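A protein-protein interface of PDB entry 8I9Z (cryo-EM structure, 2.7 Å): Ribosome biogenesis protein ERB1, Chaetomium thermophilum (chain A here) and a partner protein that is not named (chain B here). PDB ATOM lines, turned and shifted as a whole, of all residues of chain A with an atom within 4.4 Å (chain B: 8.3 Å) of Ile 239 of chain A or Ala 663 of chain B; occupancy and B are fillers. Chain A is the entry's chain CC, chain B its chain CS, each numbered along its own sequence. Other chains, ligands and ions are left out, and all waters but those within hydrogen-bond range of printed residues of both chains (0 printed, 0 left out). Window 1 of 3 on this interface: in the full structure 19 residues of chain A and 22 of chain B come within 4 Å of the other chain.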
ATOM      1  N   LEU A 231      29.994 -23.721 -27.741  1.00  0.00           N
ATOM      2  CA  LEU A 231      29.253 -22.535 -28.141  1.00  0.00           C
ATOM      3  C   LEU A 231      29.995 -21.783 -29.235  1.00  0.00           C
ATOM      4  O   LEU A 231      31.225 -21.694 -29.227  1.00  0.00           O
ATOM      5  CB  LEU A 231      29.037 -21.623 -26.940  1.00  0.00           C
ATOM      6  CG  LEU A 231      28.245 -22.197 -25.769  1.00  0.00           C
ATOM      7  CD1 LEU A 231      28.694 -21.546 -24.477  1.00  0.00           C
ATOM      8  CD2 LEU A 231      26.766 -21.974 -25.982  1.00  0.00           C
ATOM      9  N   GLU A 235      27.013 -17.085 -30.404  1.00  0.00           N
ATOM     10  CA  GLU A 235      26.292 -17.475 -29.197  1.00  0.00           C
ATOM     11  C   GLU A 235      26.926 -16.869 -27.954  1.00  0.00           C
ATOM     12  O   GLU A 235      26.219 -16.473 -27.023  1.00  0.00           O
ATOM     13  CB  GLU A 235      26.240 -18.995 -29.089  1.00  0.00           C
ATOM     14  CG  GLU A 235      25.188 -19.639 -29.968  1.00  0.00           C
ATOM     15  CD  GLU A 235      24.798 -21.022 -29.495  1.00  0.00           C
ATOM     16  OE1 GLU A 235      24.494 -21.181 -28.296  1.00  0.00           O
ATOM     17  OE2 GLU A 235      24.795 -21.955 -30.327  1.00  0.00           O
ATOM     18  N   LEU A 236      28.257 -16.789 -27.919  1.00  0.00           N
ATOM     19  CA  LEU A 236      28.934 -16.215 -26.760  1.00  0.00           C
ATOM     20  C   LEU A 236      28.665 -14.721 -26.640  1.00  0.00           C
ATOM     21  O   LEU A 236      28.642 -14.175 -25.531  1.00  0.00           O
ATOM     22  CB  LEU A 236      30.437 -16.477 -26.838  1.00  0.00           C
ATOM     23  CG  LEU A 236      30.915 -17.888 -26.508  1.00  0.00           C
ATOM     24  CD1 LEU A 236      32.214 -18.185 -27.229  1.00  0.00           C
ATOM     25  CD2 LEU A 236      31.089 -18.044 -25.012  1.00  0.00           C
ATOM     26  N   GLU A 237      28.475 -14.041 -27.770  1.00  0.00           N
ATOM     27  CA  GLU A 237      28.147 -12.622 -27.728  1.00  0.00           C
ATOM     28  C   GLU A 237      26.745 -12.400 -27.176  1.00  0.00           C
ATOM     29  O   GLU A 237      26.485 -11.396 -26.505  1.00  0.00           O
ATOM     30  CB  GLU A 237      28.288 -12.014 -29.121  1.00  0.00           C
ATOM     31  CG  GLU A 237      29.724 -11.740 -29.533  1.00  0.00           C
ATOM     32  CD  GLU A 237      30.291 -10.488 -28.893  1.00  0.00           C
ATOM     33  OE1 GLU A 237      29.503  -9.658 -28.392  1.00  0.00           O
ATOM     34  OE2 GLU A 237      31.531 -10.331 -28.892  1.00  0.00           O
ATOM     35  N   LEU A 238      25.827 -13.325 -27.456  1.00  0.00           N
ATOM     36  CA  LEU A 238      24.461 -13.200 -26.958  1.00  0.00           C
ATOM     37  C   LEU A 238      24.399 -13.408 -25.451  1.00  0.00           C
ATOM     38  O   LEU A 238      23.623 -12.743 -24.756  1.00  0.00           O
ATOM     39  CB  LEU A 238      23.553 -14.195 -27.678  1.00  0.00           C
ATOM     40  CG  LEU A 238      22.094 -14.277 -27.233  1.00  0.00           C
ATOM     41  CD1 LEU A 238      21.403 -12.945 -27.444  1.00  0.00           C
ATOM     42  CD2 LEU A 238      21.378 -15.372 -27.989  1.00  0.00           C
ATOM     43  N   ILE A 239      25.210 -14.329 -24.930  1.00  0.00           N
ATOM     44  CA  ILE A 239      25.249 -14.590 -23.493  1.00  0.00           C
ATOM     45  C   ILE A 239      25.784 -13.375 -22.750  1.00  0.00           C
ATOM     46  O   ILE A 239      25.282 -13.009 -21.680  1.00  0.00           O
ATOM     47  CB  ILE A 239      26.099 -15.842 -23.219  1.00  0.00           C
ATOM     48  CG1 ILE A 239      25.490 -17.044 -23.939  1.00  0.00           C
ATOM     49  CG2 ILE A 239      26.217 -16.102 -21.722  1.00  0.00           C
ATOM     50  CD1 ILE A 239      26.000 -18.363 -23.473  1.00  0.00           C
ATOM     51  N   ARG A 240      26.815 -12.736 -23.307  1.00  0.00           N
ATOM     52  CA  ARG A 240      27.359 -11.516 -22.724  1.00  0.00           C
ATOM     53  C   ARG A 240      26.322 -10.402 -22.706  1.00  0.00           C
ATOM     54  O   ARG A 240      26.194  -9.675 -21.715  1.00  0.00           O
ATOM     55  CB  ARG A 240      28.597 -11.086 -23.509  1.00  0.00           C
ATOM     56  CG  ARG A 240      28.976  -9.638 -23.340  1.00  0.00           C
ATOM     57  CD  ARG A 240      29.899  -9.181 -24.456  1.00  0.00           C
ATOM     58  NE  ARG A 240      29.908  -7.734 -24.660  1.00  0.00           N
ATOM     59  CZ  ARG A 240      30.322  -6.827 -23.781  1.00  0.00           C
ATOM     60  NH1 ARG A 240      30.898  -7.170 -22.640  1.00  0.00           N
ATOM     61  NH2 ARG A 240      30.183  -5.537 -24.071  1.00  0.00           N
ATOM     62  N   LYS A 241      25.555 -10.276 -23.787  1.00  0.00           N
ATOM     63  CA  LYS A 241      24.552  -9.223 -23.883  1.00  0.00           C
ATOM     64  C   LYS A 241      23.439  -9.410 -22.857  1.00  0.00           C
ATOM     65  O   LYS A 241      22.948  -8.432 -22.282  1.00  0.00           O
ATOM     66  CB  LYS A 241      23.995  -9.194 -25.305  1.00  0.00           C
ATOM     67  CG  LYS A 241      24.645  -8.147 -26.195  1.00  0.00           C
ATOM     68  CD  LYS A 241      24.128  -8.189 -27.633  1.00  0.00           C
ATOM     69  CE  LYS A 241      22.754  -7.548 -27.797  1.00  0.00           C
ATOM     70  NZ  LYS A 241      21.623  -8.455 -27.452  1.00  0.00           N
ATOM     71  N   VAL A 242      23.020 -10.655 -22.621  1.00  0.00           N
ATOM     72  CA  VAL A 242      21.955 -10.919 -21.656  1.00  0.00           C
ATOM     73  C   VAL A 242      22.459 -10.739 -20.228  1.00  0.00           C
ATOM     74  O   VAL A 242      21.762 -10.175 -19.377  1.00  0.00           O
ATOM     75  CB  VAL A 242      21.368 -12.324 -21.885  1.00  0.00           C
ATOM     76  CG1 VAL A 242      20.358 -12.677 -20.808  1.00  0.00           C
ATOM     77  CG2 VAL A 242      20.708 -12.395 -23.248  1.00  0.00           C
ATOM     78  N   GLN A 243      23.676 -11.210 -19.948  1.00  0.00           N
ATOM     79  CA  GLN A 243      24.216 -11.165 -18.592  1.00  0.00           C
ATOM     80  C   GLN A 243      24.439  -9.736 -18.117  1.00  0.00           C
ATOM     81  O   GLN A 243      23.973  -9.359 -17.038  1.00  0.00           O
ATOM     82  CB  GLN A 243      25.526 -11.953 -18.536  1.00  0.00           C
ATOM     83  CG  GLN A 243      25.987 -12.445 -17.161  1.00  0.00           C
ATOM     84  CD  GLN A 243      25.141 -13.553 -16.542  1.00  0.00           C
ATOM     85  OE1 GLN A 243      24.018 -13.835 -16.960  1.00  0.00           O
ATOM     86  NE2 GLN A 243      25.703 -14.201 -15.534  1.00  0.00           N
ATOM     87  N   ILE B 652      35.367 -13.814 -24.669  1.00  0.00           N
ATOM     88  CA  ILE B 652      34.273 -13.971 -23.722  1.00  0.00           C
ATOM     89  C   ILE B 652      34.560 -15.201 -22.877  1.00  0.00           C
ATOM     90  O   ILE B 652      34.564 -16.327 -23.388  1.00  0.00           O
ATOM     91  CB  ILE B 652      32.923 -14.098 -24.441  1.00  0.00           C
ATOM     92  CG1 ILE B 652      32.741 -12.960 -25.444  1.00  0.00           C
ATOM     93  CG2 ILE B 652      31.789 -14.102 -23.437  1.00  0.00           C
ATOM     94  CD1 ILE B 652      32.771 -11.587 -24.820  1.00  0.00           C
ATOM     95  N   ASP B 653      34.800 -14.997 -21.588  1.00  0.00           N
ATOM     96  CA  ASP B 653      35.144 -16.080 -20.679  1.00  0.00           C
ATOM     97  C   ASP B 653      33.995 -16.284 -19.701  1.00  0.00           C
ATOM     98  O   ASP B 653      33.607 -15.350 -18.992  1.00  0.00           O
ATOM     99  CB  ASP B 653      36.443 -15.770 -19.938  1.00  0.00           C
ATOM    100  CG  ASP B 653      37.225 -17.020 -19.586  1.00  0.00           C
ATOM    101  OD1 ASP B 653      36.752 -18.129 -19.911  1.00  0.00           O
ATOM    102  OD2 ASP B 653      38.311 -16.893 -18.984  1.00  0.00           O
ATOM    103  N   ILE B 654      33.457 -17.498 -19.665  1.00  0.00           N
ATOM    104  CA  ILE B 654      32.346 -17.828 -18.781  1.00  0.00           C
ATOM    105  C   ILE B 654      32.929 -18.257 -17.440  1.00  0.00           C
ATOM    106  O   ILE B 654      33.404 -19.383 -17.287  1.00  0.00           O
ATOM    107  CB  ILE B 654      31.449 -18.917 -19.379  1.00  0.00           C
ATOM    108  CG1 ILE B 654      30.898 -18.470 -20.731  1.00  0.00           C
ATOM    109  CG2 ILE B 654      30.305 -19.230 -18.441  1.00  0.00           C
ATOM    110  CD1 ILE B 654      29.994 -17.268 -20.651  1.00  0.00           C
ATOM    111  N   THR B 656      31.254 -17.092 -14.096  1.00  0.00           N
ATOM    112  CA  THR B 656      30.174 -17.265 -13.139  1.00  0.00           C
ATOM    113  C   THR B 656      29.359 -18.502 -13.482  1.00  0.00           C
ATOM    114  O   THR B 656      29.246 -18.884 -14.649  1.00  0.00           O
ATOM    115  CB  THR B 656      29.265 -16.036 -13.119  1.00  0.00           C
ATOM    116  OG1 THR B 656      28.382 -16.073 -14.244  1.00  0.00           O
ATOM    117  CG2 THR B 656      30.094 -14.765 -13.179  1.00  0.00           C
ATOM    118  N   ALA B 657      28.790 -19.129 -12.449  1.00  0.00           N
ATOM    119  CA  ALA B 657      27.957 -20.305 -12.668  1.00  0.00           C
ATOM    120  C   ALA B 657      26.630 -19.943 -13.316  1.00  0.00           C
ATOM    121  O   ALA B 657      25.994 -20.796 -13.944  1.00  0.00           O
ATOM    122  CB  ALA B 657      27.713 -21.032 -11.347  1.00  0.00           C
ATOM    123  N   GLU B 658      26.193 -18.694 -13.171  1.00  0.00           N
ATOM    124  CA  GLU B 658      24.909 -18.295 -13.730  1.00  0.00           C
ATOM    125  C   GLU B 658      25.009 -18.107 -15.240  1.00  0.00           C
ATOM    126  O   GLU B 658      24.076 -18.448 -15.978  1.00  0.00           O
ATOM    127  CB  GLU B 658      24.418 -17.030 -13.028  1.00  0.00           C
ATOM    128  CG  GLU B 658      23.528 -16.132 -13.850  1.00  0.00           C
ATOM    129  CD  GLU B 658      22.091 -16.608 -13.828  1.00  0.00           C
ATOM    130  OE1 GLU B 658      21.501 -16.635 -12.729  1.00  0.00           O
ATOM    131  OE2 GLU B 658      21.560 -16.962 -14.901  1.00  0.00           O
ATOM    132  N   ALA B 659      26.141 -17.589 -15.722  1.00  0.00           N
ATOM    133  CA  ALA B 659      26.369 -17.517 -17.161  1.00  0.00           C
ATOM    134  C   ALA B 659      26.522 -18.908 -17.765  1.00  0.00           C
ATOM    135  O   ALA B 659      26.172 -19.128 -18.931  1.00  0.00           O
ATOM    136  CB  ALA B 659      27.601 -16.665 -17.457  1.00  0.00           C
ATOM    137  N   MET B 660      27.064 -19.852 -16.992  1.00  0.00           N
ATOM    138  CA  MET B 660      27.104 -21.247 -17.419  1.00  0.00           C
ATOM    139  C   MET B 660      25.698 -21.810 -17.558  1.00  0.00           C
ATOM    140  O   MET B 660      25.419 -22.588 -18.478  1.00  0.00           O
ATOM    141  CB  MET B 660      27.909 -22.070 -16.414  1.00  0.00           C
ATOM    142  CG  MET B 660      28.789 -23.195 -16.970  1.00  0.00           C
ATOM    143  SD  MET B 660      29.707 -22.872 -18.486  1.00  0.00           S
ATOM    144  CE  MET B 660      28.694 -23.716 -19.679  1.00  0.00           C
ATOM    145  N   THR B 661      24.803 -21.431 -16.642  1.00  0.00           N
ATOM    146  CA  THR B 661      23.413 -21.874 -16.697  1.00  0.00           C
ATOM    147  C   THR B 661      22.716 -21.375 -17.953  1.00  0.00           C
ATOM    148  O   THR B 661      21.952 -22.115 -18.583  1.00  0.00           O
ATOM    149  CB  THR B 661      22.670 -21.391 -15.454  1.00  0.00           C
ATOM    150  OG1 THR B 661      23.472 -21.625 -14.290  1.00  0.00           O
ATOM    151  CG2 THR B 661      21.344 -22.094 -15.311  1.00  0.00           C
ATOM    152  N   LEU B 662      22.965 -20.123 -18.334  1.00  0.00           N
ATOM    153  CA  LEU B 662      22.408 -19.607 -19.578  1.00  0.00           C
ATOM    154  C   LEU B 662      23.054 -20.275 -20.784  1.00  0.00           C
ATOM    155  O   LEU B 662      22.428 -20.409 -21.841  1.00  0.00           O
ATOM    156  CB  LEU B 662      22.590 -18.094 -19.639  1.00  0.00           C
ATOM    157  CG  LEU B 662      21.679 -17.343 -20.601  1.00  0.00           C
ATOM    158  CD1 LEU B 662      20.261 -17.331 -20.065  1.00  0.00           C
ATOM    159  CD2 LEU B 662      22.191 -15.933 -20.814  1.00  0.00           C
ATOM    160  N   ALA B 663      24.310 -20.701 -20.643  1.00  0.00           N
ATOM    161  CA  ALA B 663      24.988 -21.396 -21.731  1.00  0.00           C
ATOM    162  C   ALA B 663      24.456 -22.811 -21.904  1.00  0.00           C
ATOM    163  O   ALA B 663      24.342 -23.301 -23.030  1.00  0.00           O
ATOM    164  CB  ALA B 663      26.492 -21.414 -21.479  1.00  0.00           C
ATOM    165  N   HIS B 664      24.144 -23.488 -20.799  1.00  0.00           N
ATOM    166  CA  HIS B 664      23.592 -24.834 -20.890  1.00  0.00           C
ATOM    167  C   HIS B 664      22.187 -24.805 -21.471  1.00  0.00           C
ATOM    168  O   HIS B 664      21.766 -25.739 -22.164  1.00  0.00           O
ATOM    169  CB  HIS B 664      23.592 -25.498 -19.516  1.00  0.00           C
ATOM    170  CG  HIS B 664      24.936 -25.990 -19.085  1.00  0.00           C
ATOM    171  ND1 HIS B 664      25.602 -26.997 -19.744  1.00  0.00           N
ATOM    172  CD2 HIS B 664      25.729 -25.628 -18.051  1.00  0.00           C
ATOM    173  CE1 HIS B 664      26.755 -27.227 -19.143  1.00  0.00           C
ATOM    174  NE2 HIS B 664      26.855 -26.410 -18.113  1.00  0.00           N
ATOM    175  N   GLN B 665      21.444 -23.734 -21.195  1.00  0.00           N
ATOM    176  CA  GLN B 665      20.094 -23.607 -21.731  1.00  0.00           C
ATOM    177  C   GLN B 665      20.120 -23.313 -23.223  1.00  0.00           C
ATOM    178  O   GLN B 665      19.314 -23.856 -23.987  1.00  0.00           O
ATOM    179  CB  GLN B 665      19.346 -22.507 -20.983  1.00  0.00           C
ATOM    180  CG  GLN B 665      18.855 -22.911 -19.612  1.00  0.00           C
ATOM    181  CD  GLN B 665      18.234 -21.754 -18.863  1.00  0.00           C
ATOM    182  OE1 GLN B 665      18.394 -20.598 -19.246  1.00  0.00           O
ATOM    183  NE2 GLN B 665      17.521 -22.059 -17.788  1.00  0.00           N
ATOM    184  N   LEU B 666      21.039 -22.451 -23.655  1.00  0.00           N
ATOM    185  CA  LEU B 666      21.078 -22.043 -25.054  1.00  0.00           C
ATOM    186  C   LEU B 666      21.661 -23.135 -25.940  1.00  0.00           C
ATOM    187  O   LEU B 666      21.178 -23.358 -27.055  1.00  0.00           O
ATOM    188  CB  LEU B 666      21.881 -20.753 -25.192  1.00  0.00           C
ATOM    189  CG  LEU B 666      21.922 -20.089 -26.565  1.00  0.00           C
ATOM    190  CD1 LEU B 666      20.523 -19.839 -27.078  1.00  0.00           C
ATOM    191  CD2 LEU B 666      22.711 -18.794 -26.498  1.00  0.00           C
ATOM    192  N   ALA B 667      22.704 -23.817 -25.465  1.00  0.00           N
ATOM    193  CA  ALA B 667      23.385 -24.807 -26.294  1.00  0.00           C
ATOM    194  C   ALA B 667      22.531 -26.052 -26.487  1.00  0.00           C
ATOM    195  O   ALA B 667      22.530 -26.652 -27.565  1.00  0.00           O
ATOM    196  CB  ALA B 667      24.731 -25.158 -25.673  1.00  0.00           C
ATOM    197  N   THR B 668      21.805 -26.458 -25.453  1.00  0.00           N
ATOM    198  CA  THR B 668      20.760 -27.456 -25.615  1.00  0.00           C
ATOM    199  C   THR B 668      19.554 -26.815 -26.294  1.00  0.00           C
ATOM    200  O   THR B 668      19.413 -25.591 -26.330  1.00  0.00           O
ATOM    201  CB  THR B 668      20.360 -28.031 -24.255  1.00  0.00           C
ATOM    202  OG1 THR B 668      21.492 -28.005 -23.383  1.00  0.00           O
ATOM    203  CG2 THR B 668      19.895 -29.474 -24.386  1.00  0.00           C
ATOM    204  N   GLY B 669      18.673 -27.649 -26.834  1.00  0.00           N
ATOM    205  CA  GLY B 669      17.469 -27.142 -27.461  1.00  0.00           C
ATOM    206  C   GLY B 669      16.373 -26.794 -26.474  1.00  0.00           C
ATOM    207  O   GLY B 669      15.233 -27.244 -26.621  1.00  0.00           O
ATOM    208  N   LYS B 671      16.316 -23.249 -24.826  1.00  0.00           N
ATOM    209  CA  LYS B 671      16.053 -21.843 -25.066  1.00  0.00           C
ATOM    210  C   LYS B 671      16.658 -21.469 -26.409  1.00  0.00           C
ATOM    211  O   LYS B 671      17.825 -21.766 -26.676  1.00  0.00           O
ATOM    212  CB  LYS B 671      16.638 -20.980 -23.952  1.00  0.00           C
ATOM    213  CG  LYS B 671      15.658 -20.668 -22.845  1.00  0.00           C
ATOM    214  CD  LYS B 671      15.864 -19.282 -22.274  1.00  0.00           C
ATOM    215  CE  LYS B 671      14.746 -18.911 -21.314  1.00  0.00           C
ATOM    216  NZ  LYS B 671      13.905 -20.082 -20.933  1.00  0.00           N
ATOM    217  N   LEU B 676      16.041 -15.780 -25.921  1.00  0.00           N
ATOM    218  CA  LEU B 676      17.049 -15.039 -25.173  1.00  0.00           C
ATOM    219  C   LEU B 676      16.959 -13.547 -25.456  1.00  0.00           C
ATOM    220  O   LEU B 676      17.128 -12.721 -24.551  1.00  0.00           O
ATOM    221  CB  LEU B 676      18.443 -15.568 -25.508  1.00  0.00           C
ATOM    222  CG  LEU B 676      19.064 -16.654 -24.623  1.00  0.00           C
ATOM    223  CD1 LEU B 676      20.559 -16.424 -24.471  1.00  0.00           C
ATOM    224  CD2 LEU B 676      18.399 -16.733 -23.261  1.00  0.00           C
ATOM    225  N   ALA B 714      25.724 -26.848 -14.259  1.00  0.00           N
ATOM    226  CA  ALA B 714      26.381 -25.587 -14.577  1.00  0.00           C
ATOM    227  C   ALA B 714      27.445 -25.247 -13.544  1.00  0.00           C
ATOM    228  O   ALA B 714      28.517 -24.740 -13.890  1.00  0.00           O
ATOM    229  CB  ALA B 714      25.348 -24.467 -14.674  1.00  0.00           C
ATOM    230  N   ILE B 718      31.817 -25.150 -13.911  1.00  0.00           N
ATOM    231  CA  ILE B 718      32.603 -23.979 -13.542  1.00  0.00           C
ATOM    232  C   ILE B 718      33.791 -24.367 -12.666  1.00  0.00           C
ATOM    233  O   ILE B 718      34.908 -23.879 -12.874  1.00  0.00           O
ATOM    234  CB  ILE B 718      31.691 -22.936 -12.874  1.00  0.00           C
ATOM    235  CG1 ILE B 718      30.816 -22.282 -13.940  1.00  0.00           C
ATOM    236  CG2 ILE B 718      32.485 -21.891 -12.126  1.00  0.00           C
ATOM    237  CD1 ILE B 718      31.604 -21.663 -15.076  1.00  0.00           C
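The backbone NH (N) of Ala 659 of chain B sits close to the side-chain amide nitrogen (NE2) of Gln 243 of chain A, 3.4 Å away.
OG1 of Thr 656 of chain B sits at hydrogen-bond distance from N of Ala 659 of chain B, at 3.1 Å.
Among the printed residues, pairs that only touch across the chains: Glu 235 of chain A with Leu 666 of chain B, Gln 243 of chain A with Glu 658 of chain B, Gln 243 of chain A with Thr 656 of chain B, Ile 239 of chain A with Ala 663 of chain B, Leu 231 of chain A with Ala 663 of chain B, Val 242 of chain A with Leu 662 of chain B, Leu 238 of chain A with Leu 676 of chain B, Arg 240 of chain A with Ile 652 of chain B, Leu 236 of chain A with Ile 652 of chain B, Leu 231 of chain A with Ala 667 of chain B, Val 242 of chain A with Leu 676 of chain B and Leu 238 of chain A with Leu 666 of chain B.
Printed residues of chain B within 4 Å of Ile 239 of chain A: Ala 663 (3.6 Å).
Of chain A, only Leu 231 and Ile 239 come within 4 Å of Ala 663 of chain B.
Of the printed residues of chain B, Arg 240 of chain A touches Ile 652.
Of the printed residues of chain A, Ala 659 of chain B touches Gln 243.
Of the printed residues of chain A, Ala 667 of chain B touches Leu 231 (3.8 Å).
Glu 237 of chain A touches none of the printed residues of chain B.
Ile 718 of chain B touches none of the printed residues of chain A.
The nearest printed residue of chain B that does not touch Ile 239 of chain A is Ile 654 of chain B (4.1 Å).
Hydrophobic or aromatic side chains of chain B that line the printed part of chain A: Ile 652, Ala 659, Leu 662, Ala 663, Leu 666, Ala 667 and Leu 676.
Among the printed residues, no Asp or Glu carboxylate lies within 4 Å of a Lys or Arg side-chain nitrogen of the other chain.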
